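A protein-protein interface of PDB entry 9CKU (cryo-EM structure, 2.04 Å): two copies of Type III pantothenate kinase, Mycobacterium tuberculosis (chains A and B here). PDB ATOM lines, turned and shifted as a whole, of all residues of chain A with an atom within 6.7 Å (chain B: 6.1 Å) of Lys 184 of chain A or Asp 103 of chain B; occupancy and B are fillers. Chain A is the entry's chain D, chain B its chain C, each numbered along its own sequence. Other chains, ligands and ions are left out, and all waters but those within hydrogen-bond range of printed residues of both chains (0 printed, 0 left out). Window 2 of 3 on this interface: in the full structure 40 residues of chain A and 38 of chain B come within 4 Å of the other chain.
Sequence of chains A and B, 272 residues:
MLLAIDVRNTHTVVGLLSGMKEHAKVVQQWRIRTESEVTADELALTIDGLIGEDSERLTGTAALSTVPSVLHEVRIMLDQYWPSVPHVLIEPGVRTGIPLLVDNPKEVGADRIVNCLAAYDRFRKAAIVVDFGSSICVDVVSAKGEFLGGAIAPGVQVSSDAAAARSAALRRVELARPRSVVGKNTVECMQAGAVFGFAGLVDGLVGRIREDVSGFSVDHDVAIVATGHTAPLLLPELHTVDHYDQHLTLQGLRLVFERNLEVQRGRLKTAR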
ATOM      1  N   ARG A 179     -20.867  16.020   4.829  1.00  0.00           N
ATOM      2  CA  ARG A 179     -20.605  14.603   4.601  1.00  0.00           C
ATOM      3  C   ARG A 179     -19.281  14.170   5.215  1.00  0.00           C
ATOM      4  O   ARG A 179     -19.183  13.077   5.782  1.00  0.00           O
ATOM      5  CB  ARG A 179     -20.612  14.290   3.105  1.00  0.00           C
ATOM      6  CG  ARG A 179     -20.416  12.812   2.802  1.00  0.00           C
ATOM      7  CD  ARG A 179     -20.414  12.433   1.311  1.00  0.00           C
ATOM      8  NE  ARG A 179     -19.317  12.969   0.510  1.00  0.00           N
ATOM      9  CZ  ARG A 179     -19.427  13.972  -0.351  1.00  0.00           C
ATOM     10  NH1 ARG A 179     -20.580  14.587  -0.559  1.00  0.00           N
ATOM     11  NH2 ARG A 179     -18.344  14.396  -0.995  1.00  0.00           N
ATOM     12  N   SER A 180     -18.250  15.001   5.102  1.00  0.00           N
ATOM     13  CA  SER A 180     -16.906  14.624   5.509  1.00  0.00           C
ATOM     14  C   SER A 180     -16.213  15.825   6.135  1.00  0.00           C
ATOM     15  O   SER A 180     -16.598  16.973   5.915  1.00  0.00           O
ATOM     16  CB  SER A 180     -16.100  14.105   4.306  1.00  0.00           C
ATOM     17  OG  SER A 180     -14.811  13.665   4.682  1.00  0.00           O
ATOM     18  N   VAL A 182     -13.272  16.585   5.300  1.00  0.00           N
ATOM     19  CA  VAL A 182     -12.548  17.142   4.163  1.00  0.00           C
ATOM     20  C   VAL A 182     -13.588  17.631   3.159  1.00  0.00           C
ATOM     21  O   VAL A 182     -14.144  16.847   2.393  1.00  0.00           O
ATOM     22  CB  VAL A 182     -11.604  16.113   3.538  1.00  0.00           C
ATOM     23  CG1 VAL A 182     -10.813  16.729   2.391  1.00  0.00           C
ATOM     24  CG2 VAL A 182     -10.672  15.537   4.584  1.00  0.00           C
ATOM     25  N   GLY A 183     -13.838  18.935   3.148  1.00  0.00           N
ATOM     26  CA  GLY A 183     -14.798  19.483   2.217  1.00  0.00           C
ATOM     27  C   GLY A 183     -14.275  19.482   0.792  1.00  0.00           C
ATOM     28  O   GLY A 183     -13.081  19.627   0.542  1.00  0.00           O
ATOM     29  N   LYS A 184     -15.193  19.302  -0.153  1.00  0.00           N
ATOM     30  CA  LYS A 184     -14.892  19.378  -1.577  1.00  0.00           C
ATOM     31  C   LYS A 184     -15.408  20.655  -2.216  1.00  0.00           C
ATOM     32  O   LYS A 184     -15.252  20.834  -3.425  1.00  0.00           O
ATOM     33  CB  LYS A 184     -15.483  18.171  -2.305  1.00  0.00           C
ATOM     34  CG  LYS A 184     -15.129  16.837  -1.693  1.00  0.00           C
ATOM     35  CD  LYS A 184     -13.648  16.548  -1.781  1.00  0.00           C
ATOM     36  CE  LYS A 184     -13.310  15.257  -1.072  1.00  0.00           C
ATOM     37  NZ  LYS A 184     -11.882  14.875  -1.234  1.00  0.00           N
ATOM     38  N   ASN A 185     -16.045  21.525  -1.440  1.00  0.00           N
ATOM     39  CA  ASN A 185     -16.463  22.839  -1.895  1.00  0.00           C
ATOM     40  C   ASN A 185     -16.519  23.733  -0.668  1.00  0.00           C
ATOM     41  O   ASN A 185     -16.440  23.260   0.466  1.00  0.00           O
ATOM     42  CB  ASN A 185     -17.812  22.802  -2.637  1.00  0.00           C
ATOM     43  CG  ASN A 185     -18.925  22.203  -1.810  1.00  0.00           C
ATOM     44  OD1 ASN A 185     -19.525  22.877  -0.976  1.00  0.00           O
ATOM     45  ND2 ASN A 185     -19.219  20.938  -2.045  1.00  0.00           N
ATOM     46  N   THR A 186     -16.657  25.032  -0.913  1.00  0.00           N
ATOM     47  CA  THR A 186     -16.492  26.019   0.150  1.00  0.00           C
ATOM     48  C   THR A 186     -17.492  25.814   1.280  1.00  0.00           C
ATOM     49  O   THR A 186     -17.131  25.914   2.457  1.00  0.00           O
ATOM     50  CB  THR A 186     -16.621  27.430  -0.421  1.00  0.00           C
ATOM     51  OG1 THR A 186     -15.576  27.657  -1.369  1.00  0.00           O
ATOM     52  CG2 THR A 186     -16.524  28.476   0.685  1.00  0.00           C
ATOM     53  N   GLU A 188     -19.039  23.056   2.199  1.00  0.00           N
ATOM     54  CA  GLU A 188     -18.650  21.877   2.966  1.00  0.00           C
ATOM     55  C   GLU A 188     -17.457  22.171   3.866  1.00  0.00           C
ATOM     56  O   GLU A 188     -17.425  21.731   5.017  1.00  0.00           O
ATOM     57  CB  GLU A 188     -18.352  20.688   2.060  1.00  0.00           C
ATOM     58  CG  GLU A 188     -19.562  20.162   1.346  1.00  0.00           C
ATOM     59  CD  GLU A 188     -19.230  19.028   0.412  1.00  0.00           C
ATOM     60  OE1 GLU A 188     -18.031  18.770   0.182  1.00  0.00           O
ATOM     61  OE2 GLU A 188     -20.175  18.396  -0.101  1.00  0.00           O
ATOM     62  N   CYS A 189     -16.449  22.875   3.347  1.00  0.00           N
ATOM     63  CA  CYS A 189     -15.272  23.176   4.158  1.00  0.00           C
ATOM     64  C   CYS A 189     -15.643  24.020   5.370  1.00  0.00           C
ATOM     65  O   CYS A 189     -15.183  23.748   6.485  1.00  0.00           O
ATOM     66  CB  CYS A 189     -14.206  23.885   3.316  1.00  0.00           C
ATOM     67  SG  CYS A 189     -13.595  22.953   1.894  1.00  0.00           S
ATOM     68  N   LEU B 100      -6.146  19.631  -8.364  1.00  0.00           N
ATOM     69  CA  LEU B 100      -7.189  20.073  -7.447  1.00  0.00           C
ATOM     70  C   LEU B 100      -8.349  19.087  -7.549  1.00  0.00           C
ATOM     71  O   LEU B 100      -9.214  19.228  -8.415  1.00  0.00           O
ATOM     72  CB  LEU B 100      -7.612  21.490  -7.823  1.00  0.00           C
ATOM     73  CG  LEU B 100      -6.799  22.671  -7.269  1.00  0.00           C
ATOM     74  CD1 LEU B 100      -7.386  23.986  -7.738  1.00  0.00           C
ATOM     75  CD2 LEU B 100      -6.677  22.663  -5.772  1.00  0.00           C
ATOM     76  N   LEU B 101      -8.376  18.095  -6.656  1.00  0.00           N
ATOM     77  CA  LEU B 101      -9.411  17.058  -6.683  1.00  0.00           C
ATOM     78  C   LEU B 101     -10.591  17.463  -5.799  1.00  0.00           C
ATOM     79  O   LEU B 101     -10.863  16.879  -4.752  1.00  0.00           O
ATOM     80  CB  LEU B 101      -8.829  15.717  -6.258  1.00  0.00           C
ATOM     81  CG  LEU B 101      -7.560  15.278  -6.991  1.00  0.00           C
ATOM     82  CD1 LEU B 101      -7.173  13.878  -6.572  1.00  0.00           C
ATOM     83  CD2 LEU B 101      -7.730  15.362  -8.496  1.00  0.00           C
ATOM     84  N   VAL B 102     -11.307  18.484  -6.256  1.00  0.00           N
ATOM     85  CA  VAL B 102     -12.471  19.015  -5.566  1.00  0.00           C
ATOM     86  C   VAL B 102     -13.583  19.230  -6.589  1.00  0.00           C
ATOM     87  O   VAL B 102     -13.429  18.930  -7.770  1.00  0.00           O
ATOM     88  CB  VAL B 102     -12.151  20.319  -4.801  1.00  0.00           C
ATOM     89  CG1 VAL B 102     -11.117  20.059  -3.710  1.00  0.00           C
ATOM     90  CG2 VAL B 102     -11.671  21.402  -5.759  1.00  0.00           C
ATOM     91  N   ASP B 103     -14.718  19.743  -6.114  1.00  0.00           N
ATOM     92  CA  ASP B 103     -15.881  19.906  -6.981  1.00  0.00           C
ATOM     93  C   ASP B 103     -15.640  20.991  -8.024  1.00  0.00           C
ATOM     94  O   ASP B 103     -15.751  20.745  -9.230  1.00  0.00           O
ATOM     95  CB  ASP B 103     -17.119  20.225  -6.142  1.00  0.00           C
ATOM     96  CG  ASP B 103     -17.545  19.062  -5.273  1.00  0.00           C
ATOM     97  OD1 ASP B 103     -16.980  17.961  -5.431  1.00  0.00           O
ATOM     98  OD2 ASP B 103     -18.440  19.251  -4.425  1.00  0.00           O
ATOM     99  N   ASN B 104     -15.318  22.202  -7.579  1.00  0.00           N
ATOM    100  CA  ASN B 104     -15.079  23.334  -8.473  1.00  0.00           C
ATOM    101  C   ASN B 104     -13.681  23.864  -8.197  1.00  0.00           C
ATOM    102  O   ASN B 104     -13.493  24.656  -7.256  1.00  0.00           O
ATOM    103  CB  ASN B 104     -16.122  24.431  -8.277  1.00  0.00           C
ATOM    104  CG  ASN B 104     -15.960  25.575  -9.259  1.00  0.00           C
ATOM    105  OD1 ASN B 104     -15.314  25.437 -10.296  1.00  0.00           O
ATOM    106  ND2 ASN B 104     -16.555  26.716  -8.934  1.00  0.00           N
ATOM    107  N   PRO B 105     -12.672  23.469  -8.979  1.00  0.00           N
ATOM    108  CA  PRO B 105     -11.308  23.936  -8.691  1.00  0.00           C
ATOM    109  C   PRO B 105     -11.174  25.444  -8.677  1.00  0.00           C
ATOM    110  O   PRO B 105     -10.322  25.971  -7.956  1.00  0.00           O
ATOM    111  CB  PRO B 105     -10.480  23.306  -9.817  1.00  0.00           C
ATOM    112  CG  PRO B 105     -11.244  22.102 -10.210  1.00  0.00           C
ATOM    113  CD  PRO B 105     -12.687  22.457 -10.049  1.00  0.00           C
ATOM    114  N   GLU B 107     -12.893  27.607  -7.272  1.00  0.00           N
ATOM    115  CA  GLU B 107     -13.276  28.229  -6.010  1.00  0.00           C
ATOM    116  C   GLU B 107     -12.255  28.005  -4.901  1.00  0.00           C
ATOM    117  O   GLU B 107     -12.469  28.482  -3.784  1.00  0.00           O
ATOM    118  CB  GLU B 107     -14.661  27.730  -5.554  1.00  0.00           C
ATOM    119  CG  GLU B 107     -14.690  26.460  -4.703  1.00  0.00           C
ATOM    120  CD  GLU B 107     -16.102  26.090  -4.268  1.00  0.00           C
ATOM    121  OE1 GLU B 107     -16.857  27.003  -3.870  1.00  0.00           O
ATOM    122  OE2 GLU B 107     -16.461  24.900  -4.338  1.00  0.00           O
ATOM    123  N   LEU B 148      -6.777  17.440  -1.808  1.00  0.00           N
ATOM    124  CA  LEU B 148      -8.028  16.732  -1.576  1.00  0.00           C
ATOM    125  C   LEU B 148      -9.138  17.622  -1.026  1.00  0.00           C
ATOM    126  O   LEU B 148     -10.304  17.227  -1.084  1.00  0.00           O
ATOM    127  CB  LEU B 148      -7.787  15.562  -0.619  1.00  0.00           C
ATOM    128  CG  LEU B 148      -6.863  14.465  -1.162  1.00  0.00           C
ATOM    129  CD1 LEU B 148      -6.578  13.423  -0.093  1.00  0.00           C
ATOM    130  CD2 LEU B 148      -7.414  13.824  -2.426  1.00  0.00           C
ATOM    131  N   GLY B 149      -8.815  18.811  -0.518  1.00  0.00           N
ATOM    132  CA  GLY B 149      -9.774  19.666   0.147  1.00  0.00           C
ATOM    133  C   GLY B 149      -9.382  19.911   1.594  1.00  0.00           C
ATOM    134  O   GLY B 149      -8.198  19.873   1.947  1.00  0.00           O
ATOM    135  N   GLY B 150     -10.385  20.157   2.423  1.00  0.00           N
ATOM    136  CA  GLY B 150     -10.108  20.365   3.832  1.00  0.00           C
ATOM    137  C   GLY B 150     -11.251  21.077   4.533  1.00  0.00           C
ATOM    138  O   GLY B 150     -12.410  20.946   4.149  1.00  0.00           O
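O of Lys 184 of chain A is in hydrogen-bond range of N of Asp 103 of chain B (3.0 Å).
The backbone carbonyl oxygen (O) of Gly 150 of chain B sits at hydrogen-bond distance from the backbone NH (N) of Gly 183 of chain A, at 2.7 Å.
NZ of Lys 184 of chain A sits at hydrogen-bond distance from O of Leu 148 of chain B (2.8 Å).
OD2 of Asp 103 of chain B sits at hydrogen-bond distance from ND2 of Asn 185 of chain A (3.0 Å).
The side-chain sulfur (SG) of Cys 189 of chain A is in hydrogen-bond range of the backbone carbonyl oxygen (O) of Gly 150 of chain B (3.2 Å).
The side-chain carboxylate of Glu 107 of chain B sits at hydrogen-bond distance from the side-chain hydroxyl of Thr 186 of chain A (2.9 Å).
The backbone carbonyl oxygen of Gly 183 of chain A lies within hydrogen-bond range of the side-chain sulfur of Cys 189 of chain A.
The side-chain amide oxygen of Asn 185 of chain A is in hydrogen-bond range of the backbone NH of Glu 188 of chain A (3.2 Å).
OE1 of Glu 188 of chain A sits at hydrogen-bond distance from N of Lys 184 of chain A, at 2.9 Å.
The backbone NH of Val 182 of chain A lies close to the side-chain hydroxyl of Ser 180 of chain A (3.4 Å).
SG of Cys 189 of chain A lies within hydrogen-bond range of O of Asn 185 of chain A (3.2 Å).
Leu 148 of chain B touches Val 182 of chain A (O to CG1, 3.5 Å).
Val 182 of chain A touches Gly 149 of chain B (CG1 to C, 3.6 Å).
Val 182 of chain A touches Gly 150 of chain B (CG1 to N, 3.5 Å).
Gly 183 of chain A touches Gly 149 of chain B.
CB of Val 102 of chain B touches O of Lys 184 of chain A, at 3.4 Å.
Glu 107 of chain B touches Asn 185 of chain A (OE2 to CB, 3.0 Å).
Ser 180 of chain A touches none of the printed residues of chain B.
Of the printed residues of chain B, Gly 183 of chain A touches Gly 149 (3.3 Å) and Gly 150 (2.7 Å).
Lys 184 of chain A touches three residues of chain B.
Of the printed residues of chain B, Cys 189 of chain A touches Gly 150 (3.2 Å).
Printed residues of chain A within 4 Å of Val 102 of chain B: Lys 184.
Asp 103 of chain B touches just these residues of chain A: Lys 184 and Asn 185.
Of the printed residues of chain A, Gly 149 of chain B touches Val 182 and Gly 183.
The nearest residue of chain B that does not touch Lys 184 of chain A is Leu 101 of chain B (4.1 Å).
The nearest residue of chain A that does not touch Asp 103 of chain B is Glu 188 of chain A (4.7 Å).
The nearest printed residue of chain B that does not touch Thr 186 of chain A is Asn 104 of chain B (6.9 Å).
Of the 9 printed residues of chain A, 6 touch a printed residue of chain B.
Printed residues of chain A that touch a printed residue of chain B: Val 182, Gly 183, Lys 184, Asn 185, Thr 186 and Cys 189.
Hydrophobic or aromatic side chains of chain A within 4 Å of the printed part of chain B: Val 182.
Among the printed residues, 12 pairs touch across the chains.
No position is printed for both chains.
Of the 12 pairs that touch across the chains among the printed residues, none has its exchanged pair printed and touching as well.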
